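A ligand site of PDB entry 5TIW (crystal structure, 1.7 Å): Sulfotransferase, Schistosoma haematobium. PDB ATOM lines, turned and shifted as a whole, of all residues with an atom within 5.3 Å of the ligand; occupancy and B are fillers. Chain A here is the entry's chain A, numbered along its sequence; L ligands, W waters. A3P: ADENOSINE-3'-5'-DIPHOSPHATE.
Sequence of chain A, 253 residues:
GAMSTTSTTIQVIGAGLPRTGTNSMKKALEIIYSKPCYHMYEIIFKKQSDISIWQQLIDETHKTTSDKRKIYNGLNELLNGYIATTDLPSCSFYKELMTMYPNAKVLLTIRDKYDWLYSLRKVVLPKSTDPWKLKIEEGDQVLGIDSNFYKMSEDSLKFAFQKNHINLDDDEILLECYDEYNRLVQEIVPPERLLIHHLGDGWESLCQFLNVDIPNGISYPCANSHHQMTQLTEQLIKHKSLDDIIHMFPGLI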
ATOM      1  N   LEU A  17       9.450  -1.231  16.889  1.00  0.00           N
ATOM      2  CA  LEU A  17      10.229  -2.315  16.314  1.00  0.00           C
ATOM      3  C   LEU A  17       9.354  -3.194  15.421  1.00  0.00           C
ATOM      4  O   LEU A  17       8.146  -3.175  15.501  1.00  0.00           O
ATOM      5  CB  LEU A  17      10.857  -3.123  17.445  1.00  0.00           C
ATOM      6  CG  LEU A  17      11.955  -2.388  18.214  1.00  0.00           C
ATOM      7  CD1 LEU A  17      12.263  -3.077  19.538  1.00  0.00           C
ATOM      8  CD2 LEU A  17      13.218  -2.312  17.359  1.00  0.00           C
ATOM      9  N   PRO A  18       9.971  -4.029  14.582  1.00  0.00           N
ATOM     10  CA  PRO A  18       9.186  -4.991  13.799  1.00  0.00           C
ATOM     11  C   PRO A  18       8.345  -5.865  14.705  1.00  0.00           C
ATOM     12  O   PRO A  18       8.733  -6.176  15.836  1.00  0.00           O
ATOM     13  CB  PRO A  18      10.254  -5.825  13.071  1.00  0.00           C
ATOM     14  CG  PRO A  18      11.490  -5.516  13.725  1.00  0.00           C
ATOM     15  CD  PRO A  18      11.400  -4.154  14.264  1.00  0.00           C
ATOM     16  N   ARG A  19       7.190  -6.254  14.184  1.00  0.00           N
ATOM     17  CA  ARG A  19       6.217  -7.101  14.861  1.00  0.00           C
ATOM     18  C   ARG A  19       5.499  -6.422  16.023  1.00  0.00           C
ATOM     19  O   ARG A  19       5.025  -7.097  16.941  1.00  0.00           O
ATOM     20  CB  ARG A  19       6.814  -8.441  15.313  1.00  0.00           C
ATOM     21  CG  ARG A  19       7.602  -9.170  14.189  1.00  0.00           C
ATOM     22  CD  ARG A  19       6.824  -9.286  12.873  1.00  0.00           C
ATOM     23  NE  ARG A  19       5.617 -10.094  12.997  1.00  0.00           N
ATOM     24  CZ  ARG A  19       4.709 -10.236  12.049  1.00  0.00           C
ATOM     25  NH1 ARG A  19       4.842  -9.596  10.878  1.00  0.00           N
ATOM     26  NH2 ARG A  19       3.664 -11.017  12.235  1.00  0.00           N
ATOM     27  N   THR A  20       5.364  -5.090  15.994  1.00  0.00           N
ATOM     28  CA  THR A  20       4.604  -4.316  16.978  1.00  0.00           C
ATOM     29  C   THR A  20       3.388  -3.618  16.367  1.00  0.00           C
ATOM     30  O   THR A  20       2.883  -2.647  16.952  1.00  0.00           O
ATOM     31  CB  THR A  20       5.483  -3.280  17.701  1.00  0.00           C
ATOM     32  OG1 THR A  20       5.985  -2.325  16.771  1.00  0.00           O
ATOM     33  CG2 THR A  20       6.682  -3.935  18.454  1.00  0.00           C
ATOM     34  N   GLY A  21       2.961  -4.008  15.173  1.00  0.00           N
ATOM     35  CA  GLY A  21       1.847  -3.367  14.516  1.00  0.00           C
ATOM     36  C   GLY A  21       2.268  -2.318  13.511  1.00  0.00           C
ATOM     37  O   GLY A  21       1.473  -1.407  13.228  1.00  0.00           O
ATOM     38  N   THR A  22       3.493  -2.397  12.990  1.00  0.00           N
ATOM     39  CA  THR A  22       3.999  -1.361  12.082  1.00  0.00           C
ATOM     40  C   THR A  22       3.290  -1.363  10.735  1.00  0.00           C
ATOM     41  O   THR A  22       3.102  -0.296  10.151  1.00  0.00           O
ATOM     42  CB  THR A  22       5.502  -1.465  11.850  1.00  0.00           C
ATOM     43  OG1 THR A  22       5.818  -2.670  11.159  1.00  0.00           O
ATOM     44  CG2 THR A  22       6.279  -1.431  13.182  1.00  0.00           C
ATOM     45  N   ASN A  23       2.894  -2.513  10.226  1.00  0.00           N
ATOM     46  CA  ASN A  23       2.246  -2.515   8.919  1.00  0.00           C
ATOM     47  C   ASN A  23       0.838  -1.956   9.024  1.00  0.00           C
ATOM     48  O   ASN A  23       0.390  -1.213   8.140  1.00  0.00           O
ATOM     49  CB  ASN A  23       2.218  -3.906   8.318  1.00  0.00           C
ATOM     50  CG  ASN A  23       1.781  -3.911   6.878  1.00  0.00           C
ATOM     51  OD1 ASN A  23       0.655  -4.277   6.561  1.00  0.00           O
ATOM     52  ND2 ASN A  23       2.676  -3.487   5.995  1.00  0.00           N
ATOM     53  N   SER A  24       0.129  -2.296  10.102  1.00  0.00           N
ATOM     54  CA  SER A  24      -1.173  -1.667  10.297  1.00  0.00           C
ATOM     55  C   SER A  24      -1.016  -0.161  10.463  1.00  0.00           C
ATOM     56  O   SER A  24      -1.851   0.619   9.996  1.00  0.00           O
ATOM     57  CB  SER A  24      -1.885  -2.262  11.517  1.00  0.00           C
ATOM     58  OG  SER A  24      -2.212  -3.627  11.333  1.00  0.00           O
ATOM     59  N   HIS A  39       7.910   1.245   4.810  1.00  0.00           N
ATOM     60  CA  HIS A  39       7.821   0.030   5.606  1.00  0.00           C
ATOM     61  C   HIS A  39       8.749  -0.995   4.961  1.00  0.00           C
ATOM     62  O   HIS A  39       9.132  -0.831   3.798  1.00  0.00           O
ATOM     63  CB  HIS A  39       6.381  -0.478   5.616  1.00  0.00           C
ATOM     64  CG  HIS A  39       6.140  -1.595   6.560  1.00  0.00           C
ATOM     65  ND1 HIS A  39       6.185  -2.924   6.173  1.00  0.00           N
ATOM     66  CD2 HIS A  39       5.803  -1.593   7.868  1.00  0.00           C
ATOM     67  CE1 HIS A  39       5.951  -3.688   7.228  1.00  0.00           C
ATOM     68  NE2 HIS A  39       5.706  -2.911   8.266  1.00  0.00           N
ATOM     69  N   ASP A  87       8.759   0.589  10.767  1.00  0.00           N
ATOM     70  CA  ASP A  87       9.419  -0.714  10.657  1.00  0.00           C
ATOM     71  C   ASP A  87      10.922  -0.590  10.484  1.00  0.00           C
ATOM     72  O   ASP A  87      11.463   0.498  10.264  1.00  0.00           O
ATOM     73  CB  ASP A  87       8.843  -1.514   9.483  1.00  0.00           C
ATOM     74  CG  ASP A  87       9.016  -3.020   9.602  1.00  0.00           C
ATOM     75  OD1 ASP A  87       9.493  -3.549  10.638  1.00  0.00           O
ATOM     76  OD2 ASP A  87       8.644  -3.707   8.613  1.00  0.00           O
ATOM     77  N   ARG A 111       4.083  -3.684  22.301  1.00  0.00           N
ATOM     78  CA  ARG A 111       3.236  -4.799  22.708  1.00  0.00           C
ATOM     79  C   ARG A 111       3.956  -5.600  23.786  1.00  0.00           C
ATOM     80  O   ARG A 111       5.121  -5.364  24.102  1.00  0.00           O
ATOM     81  CB  ARG A 111       2.907  -5.712  21.528  1.00  0.00           C
ATOM     82  CG  ARG A 111       4.082  -6.530  21.042  1.00  0.00           C
ATOM     83  CD  ARG A 111       3.798  -7.286  19.778  1.00  0.00           C
ATOM     84  NE  ARG A 111       2.755  -8.305  19.902  1.00  0.00           N
ATOM     85  CZ  ARG A 111       2.477  -9.163  18.938  1.00  0.00           C
ATOM     86  NH1 ARG A 111       3.173  -9.176  17.809  1.00  0.00           N
ATOM     87  NH2 ARG A 111       1.481 -10.004  19.113  1.00  0.00           N
ATOM     88  N   ASP A 115       4.868 -12.014  23.502  1.00  0.00           N
ATOM     89  CA  ASP A 115       4.158 -12.095  22.225  1.00  0.00           C
ATOM     90  C   ASP A 115       5.047 -11.565  21.093  1.00  0.00           C
ATOM     91  O   ASP A 115       5.133 -12.171  20.019  1.00  0.00           O
ATOM     92  CB  ASP A 115       2.884 -11.258  22.276  1.00  0.00           C
ATOM     93  CG  ASP A 115       1.803 -11.789  23.188  1.00  0.00           C
ATOM     94  OD1 ASP A 115       1.823 -12.960  23.584  1.00  0.00           O
ATOM     95  OD2 ASP A 115       0.916 -10.979  23.510  1.00  0.00           O
ATOM     96  N   SER A 119       6.511 -13.630  17.730  1.00  0.00           N
ATOM     97  CA  SER A 119       6.199 -13.103  16.401  1.00  0.00           C
ATOM     98  C   SER A 119       7.487 -12.860  15.615  1.00  0.00           C
ATOM     99  O   SER A 119       7.559 -13.168  14.419  1.00  0.00           O
ATOM    100  CB  SER A 119       5.375 -11.815  16.573  1.00  0.00           C
ATOM    101  OG  SER A 119       4.890 -11.322  15.352  1.00  0.00           O
ATOM    102  N   VAL A 123       8.586 -14.940  12.049  1.00  0.00           N
ATOM    103  CA  VAL A 123       8.464 -14.174  10.814  1.00  0.00           C
ATOM    104  C   VAL A 123       9.803 -13.633  10.360  1.00  0.00           C
ATOM    105  O   VAL A 123      10.140 -13.711   9.177  1.00  0.00           O
ATOM    106  CB  VAL A 123       7.425 -13.033  10.954  1.00  0.00           C
ATOM    107  CG1 VAL A 123       7.380 -12.168   9.704  1.00  0.00           C
ATOM    108  CG2 VAL A 123       6.027 -13.594  11.270  1.00  0.00           C
ATOM    109  N   LEU A 199      -0.582  -2.153  20.928  1.00  0.00           N
ATOM    110  CA  LEU A 199      -1.292  -3.004  20.001  1.00  0.00           C
ATOM    111  C   LEU A 199      -2.740  -3.155  20.445  1.00  0.00           C
ATOM    112  O   LEU A 199      -3.011  -3.415  21.617  1.00  0.00           O
ATOM    113  CB  LEU A 199      -0.555  -4.337  19.966  1.00  0.00           C
ATOM    114  CG  LEU A 199      -0.781  -5.191  18.744  1.00  0.00           C
ATOM    115  CD1 LEU A 199      -0.382  -4.423  17.503  1.00  0.00           C
ATOM    116  CD2 LEU A 199       0.019  -6.483  18.847  1.00  0.00           C
ATOM    117  N   GLY A 200      -3.663  -2.899  19.525  1.00  0.00           N
ATOM    118  CA  GLY A 200      -5.087  -2.918  19.792  1.00  0.00           C
ATOM    119  C   GLY A 200      -5.732  -1.547  20.031  1.00  0.00           C
ATOM    120  O   GLY A 200      -6.956  -1.470  20.026  1.00  0.00           O
ATOM    121  N   TYR A 220      -9.772   0.480  11.856  1.00  0.00           N
ATOM    122  CA  TYR A 220      -8.336   0.580  11.994  1.00  0.00           C
ATOM    123  C   TYR A 220      -7.719  -0.714  11.480  1.00  0.00           C
ATOM    124  O   TYR A 220      -8.239  -1.797  11.763  1.00  0.00           O
ATOM    125  CB  TYR A 220      -7.950   0.757  13.464  1.00  0.00           C
ATOM    126  CG  TYR A 220      -6.445   0.973  13.624  1.00  0.00           C
ATOM    127  CD1 TYR A 220      -5.871   2.252  13.563  1.00  0.00           C
ATOM    128  CD2 TYR A 220      -5.598  -0.096  13.838  1.00  0.00           C
ATOM    129  CE1 TYR A 220      -4.517   2.444  13.693  1.00  0.00           C
ATOM    130  CE2 TYR A 220      -4.232   0.080  13.955  1.00  0.00           C
ATOM    131  CZ  TYR A 220      -3.691   1.346  13.881  1.00  0.00           C
ATOM    132  OH  TYR A 220      -2.332   1.497  13.974  1.00  0.00           O
ATOM    133  N   PRO A 221      -6.651  -0.640  10.691  1.00  0.00           N
ATOM    134  CA  PRO A 221      -6.135  -1.859  10.049  1.00  0.00           C
ATOM    135  C   PRO A 221      -5.678  -2.934  11.025  1.00  0.00           C
ATOM    136  O   PRO A 221      -5.203  -2.665  12.133  1.00  0.00           O
ATOM    137  CB  PRO A 221      -4.985  -1.343   9.195  1.00  0.00           C
ATOM    138  CG  PRO A 221      -5.283   0.141   8.995  1.00  0.00           C
ATOM    139  CD  PRO A 221      -5.885   0.548  10.299  1.00  0.00           C
ATOM    140  N   CYS A 222      -5.783  -4.201  10.578  1.00  0.00           N
ATOM    141  CA  CYS A 222      -5.347  -5.332  11.389  1.00  0.00           C
ATOM    142  C   CYS A 222      -4.623  -6.274  10.427  1.00  0.00           C
ATOM    143  O   CYS A 222      -5.178  -7.226   9.899  1.00  0.00           O
ATOM    144  CB  CYS A 222      -6.506  -6.020  12.107  1.00  0.00           C
ATOM    145  SG  CYS A 222      -5.947  -7.314  13.190  1.00  0.00           S
ATOM    146  N   ALA A 223      -3.366  -5.948  10.164  1.00  0.00           N
ATOM    147  CA  ALA A 223      -2.603  -6.517   9.058  1.00  0.00           C
ATOM    148  C   ALA A 223      -1.374  -7.265   9.569  1.00  0.00           C
ATOM    149  O   ALA A 223      -0.822  -6.946  10.616  1.00  0.00           O
ATOM    150  CB  ALA A 223      -2.112  -5.415   8.105  1.00  0.00           C
ATOM    151  N   ASN A 224      -0.938  -8.248   8.789  1.00  0.00           N
ATOM    152  CA  ASN A 224       0.436  -8.745   8.885  1.00  0.00           C
ATOM    153  C   ASN A 224       0.601  -9.695  10.057  1.00  0.00           C
ATOM    154  O   ASN A 224       1.660  -9.701  10.689  1.00  0.00           O
ATOM    155  CB  ASN A 224       1.441  -7.585   8.989  1.00  0.00           C
ATOM    156  CG  ASN A 224       2.880  -7.985   8.597  1.00  0.00           C
ATOM    157  OD1 ASN A 224       3.120  -8.976   7.896  1.00  0.00           O
ATOM    158  ND2 ASN A 224       3.847  -7.170   8.983  1.00  0.00           N
ATOM    159  N   SER A 225      -0.385 -10.536  10.330  1.00  0.00           N
ATOM    160  CA  SER A 225      -0.255 -11.494  11.438  1.00  0.00           C
ATOM    161  C   SER A 225       0.741 -12.598  11.098  1.00  0.00           C
ATOM    162  O   SER A 225       1.002 -12.922   9.921  1.00  0.00           O
ATOM    163  CB  SER A 225      -1.596 -12.125  11.746  1.00  0.00           C
ATOM    164  OG  SER A 225      -1.994 -12.979  10.689  1.00  0.00           O
ATOM    165  N   HIS A 226       1.283 -13.244  12.140  1.00  0.00           N
ATOM    166  CA  HIS A 226       2.237 -14.312  11.857  1.00  0.00           C
ATOM    167  C   HIS A 226       1.545 -15.458  11.140  1.00  0.00           C
ATOM    168  O   HIS A 226       2.172 -16.114  10.290  1.00  0.00           O
ATOM    169  CB  HIS A 226       2.997 -14.784  13.106  1.00  0.00           C
ATOM    170  CG  HIS A 226       2.146 -15.483  14.126  1.00  0.00           C
ATOM    171  ND1 HIS A 226       1.707 -16.780  13.983  1.00  0.00           N
ATOM    172  CD2 HIS A 226       1.727 -15.084  15.360  1.00  0.00           C
ATOM    173  CE1 HIS A 226       1.012 -17.144  15.047  1.00  0.00           C
ATOM    174  NE2 HIS A 226       0.988 -16.122  15.897  1.00  0.00           N
ATOM    175  N   HIS A 227       0.269 -15.701  11.432  1.00  0.00           N
ATOM    176  CA  HIS A 227      -0.448 -16.759  10.724  1.00  0.00           C
ATOM    177  C   HIS A 227      -0.486 -16.468   9.225  1.00  0.00           C
ATOM    178  O   HIS A 227      -0.218 -17.343   8.394  1.00  0.00           O
ATOM    179  CB  HIS A 227      -1.872 -16.907  11.267  1.00  0.00           C
ATOM    180  CG  HIS A 227      -2.688 -17.919  10.518  1.00  0.00           C
ATOM    181  ND1 HIS A 227      -2.444 -19.275  10.596  1.00  0.00           N
ATOM    182  CD2 HIS A 227      -3.736 -17.774   9.681  1.00  0.00           C
ATOM    183  CE1 HIS A 227      -3.321 -19.917   9.832  1.00  0.00           C
ATOM    184  NE2 HIS A 227      -4.115 -19.028   9.264  1.00  0.00           N
HETATM  185  P1  A3P L   1       1.312 -11.476  15.481  1.00  0.00           P
HETATM  186  O1P A3P L   1       2.491 -11.905  14.751  1.00  0.00           O
HETATM  187  O2P A3P L   1       1.346 -11.879  16.954  1.00  0.00           O
HETATM  188  O3P A3P L   1       0.075 -11.946  14.792  1.00  0.00           O
HETATM  189  P2  A3P L   1       4.312  -5.710  12.189  1.00  0.00           P
HETATM  190  O4P A3P L   1       5.214  -6.789  11.681  1.00  0.00           O
HETATM  191  O5P A3P L   1       5.065  -4.639  12.881  1.00  0.00           O
HETATM  192  O6P A3P L   1       3.370  -5.244  11.087  1.00  0.00           O
HETATM  193  O5' A3P L   1       3.288  -6.245  13.372  1.00  0.00           O
HETATM  194  C5' A3P L   1       2.537  -7.390  13.112  1.00  0.00           C
HETATM  195  C4' A3P L   1       1.908  -7.918  14.443  1.00  0.00           C
HETATM  196  O4' A3P L   1       0.922  -6.839  14.864  1.00  0.00           O
HETATM  197  C3' A3P L   1       1.231  -9.061  14.292  1.00  0.00           C
HETATM  198  O3' A3P L   1       1.257  -9.845  15.517  1.00  0.00           O
HETATM  199  C2' A3P L   1      -0.291  -8.568  14.045  1.00  0.00           C
HETATM  200  O2' A3P L   1      -1.269  -9.631  14.306  1.00  0.00           O
HETATM  201  C1' A3P L   1      -0.387  -7.610  14.936  1.00  0.00           C
HETATM  202  N9  A3P L   1      -1.453  -6.620  14.744  1.00  0.00           N
HETATM  203  C8  A3P L   1      -1.368  -5.791  13.683  1.00  0.00           C
HETATM  204  N7  A3P L   1      -2.444  -4.977  13.743  1.00  0.00           N
HETATM  205  C5  A3P L   1      -3.123  -5.294  14.839  1.00  0.00           C
HETATM  206  C6  A3P L   1      -4.247  -4.778  15.384  1.00  0.00           C
HETATM  207  N6  A3P L   1      -5.134  -3.757  14.970  1.00  0.00           N
HETATM  208  N1  A3P L   1      -4.726  -5.285  16.504  1.00  0.00           N
HETATM  209  C2  A3P L   1      -4.089  -6.322  17.111  1.00  0.00           C
HETATM  210  N3  A3P L   1      -2.952  -6.845  16.594  1.00  0.00           N
HETATM  211  C4  A3P L   1      -2.510  -6.288  15.460  1.00  0.00           C
HETATM  212  O   HOH W   1      -0.967 -12.646  18.199  1.00  0.00           O
HETATM  213  O   HOH W   2       0.749  -4.727  11.415  1.00  0.00           O
HETATM  214  O   HOH W   3       2.875 -13.377  18.774  1.00  0.00           O
HETATM  215  O   HOH W   4      -2.362  -9.430  18.113  1.00  0.00           O
HETATM  216  O   HOH W   5      -7.530  -2.272  16.095  1.00  0.00           O
HETATM  217  O   HOH W   6      -7.275  -5.256  17.668  1.00  0.00           O
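C of Pro 18 touches O5P of the ligand, at 3.9 Å.
CG of Leu 199 touches N3 of the ligand, at 3.5 Å.
Gly 200 touches the ligand (N to N1, 3.99 Å).
Tyr 220 touches the ligand (CD2 to N6, 3.9 Å).
Cys 222 touches the ligand.
O of Ala 223 touches C8 of the ligand (3.3 Å).
CA of Ser 225 touches O3P of the ligand, at 3.4 Å.
Hydrophobic or aromatic side chains within 4 Å of the ligand: Leu 199, Tyr 220 and His 226.
Of the 24 residues printed, 18 come within 4 Å of the ligand.
The side-chain hydroxyl (OG) of Ser 119 sits at hydrogen-bond distance from the guanidinium group (NE) of Arg 19 (2.8 Å).
A ring nitrogen (NE2) of His 39 lies within hydrogen-bond range of the side-chain hydroxyl (OG1) of Thr 22.
OG of Ser 24 lies within hydrogen-bond range of O of Pro 221 (3.2 Å).
The side-chain hydroxyl (OG) of Ser 24 sits at hydrogen-bond distance from the backbone NH (N) of Ala 223 (2.8 Å).
The backbone carbonyl oxygen (O) of Arg 19 lies within hydrogen-bond range of the guanidinium group (NH1) of Arg 111, 2.9 Å away.
The backbone carbonyl oxygen (O) of Asn 224 is in hydrogen-bond range of the guanidinium group (NH2) of Arg 19.
The backbone NH of Asn 23 is in hydrogen-bond range of a ring nitrogen (NE2) of His 39 (3.5 Å).
OG1 of Thr 20 lies within hydrogen-bond range of O of Leu 17, at 2.6 Å.
Water W2 lies within hydrogen-bond range of O6P of the ligand (2.7 Å), N of Ser 24 (2.8 Å), O of Ala 223 (2.8 Å) and N of Asn 23 (3.3 Å).
Water W3 lies within hydrogen-bond range of O2P of the ligand (2.8 Å) and O of Asp 115 (2.8 Å).
The side-chain hydroxyl of Ser 119 sits at hydrogen-bond distance from an oxygen (O1P) of the ligand, at 2.5 Å.
The backbone NH of Thr 22 sits at hydrogen-bond distance from an oxygen (O5P) of the ligand, 2.7 Å away.
O5P of the ligand lies within hydrogen-bond range of OG1 of Thr 22.
The side-chain hydroxyl (OG) of Ser 24 is in hydrogen-bond range of a nitrogen (N7) of the ligand.
The guanidinium group (NH2) of Arg 111 lies within salt-bridge range of an oxygen (O2P) of the ligand.
The backbone NH of Gly 21 sits at hydrogen-bond distance from an oxygen (O5') of the ligand, 2.9 Å away.
O6P of the ligand sits at hydrogen-bond distance from ND2 of Asn 224, 2.9 Å away.
The backbone NH (N) of Asn 23 sits at hydrogen-bond distance from an oxygen (O6P) of the ligand (2.9 Å).
The backbone NH of Arg 19 sits at hydrogen-bond distance from an oxygen (O5P) of the ligand.
O1P of the ligand lies within salt-bridge range of NH2 of Arg 19.
The backbone carbonyl oxygen (O) of Pro 221 is in hydrogen-bond range of a nitrogen (N6) of the ligand, at 3.0 Å.
The backbone NH of Thr 20 is in hydrogen-bond range of an oxygen (O5P) of the ligand (3.2 Å).
The backbone NH (N) of His 226 is in hydrogen-bond range of an oxygen (O1P) of the ligand.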
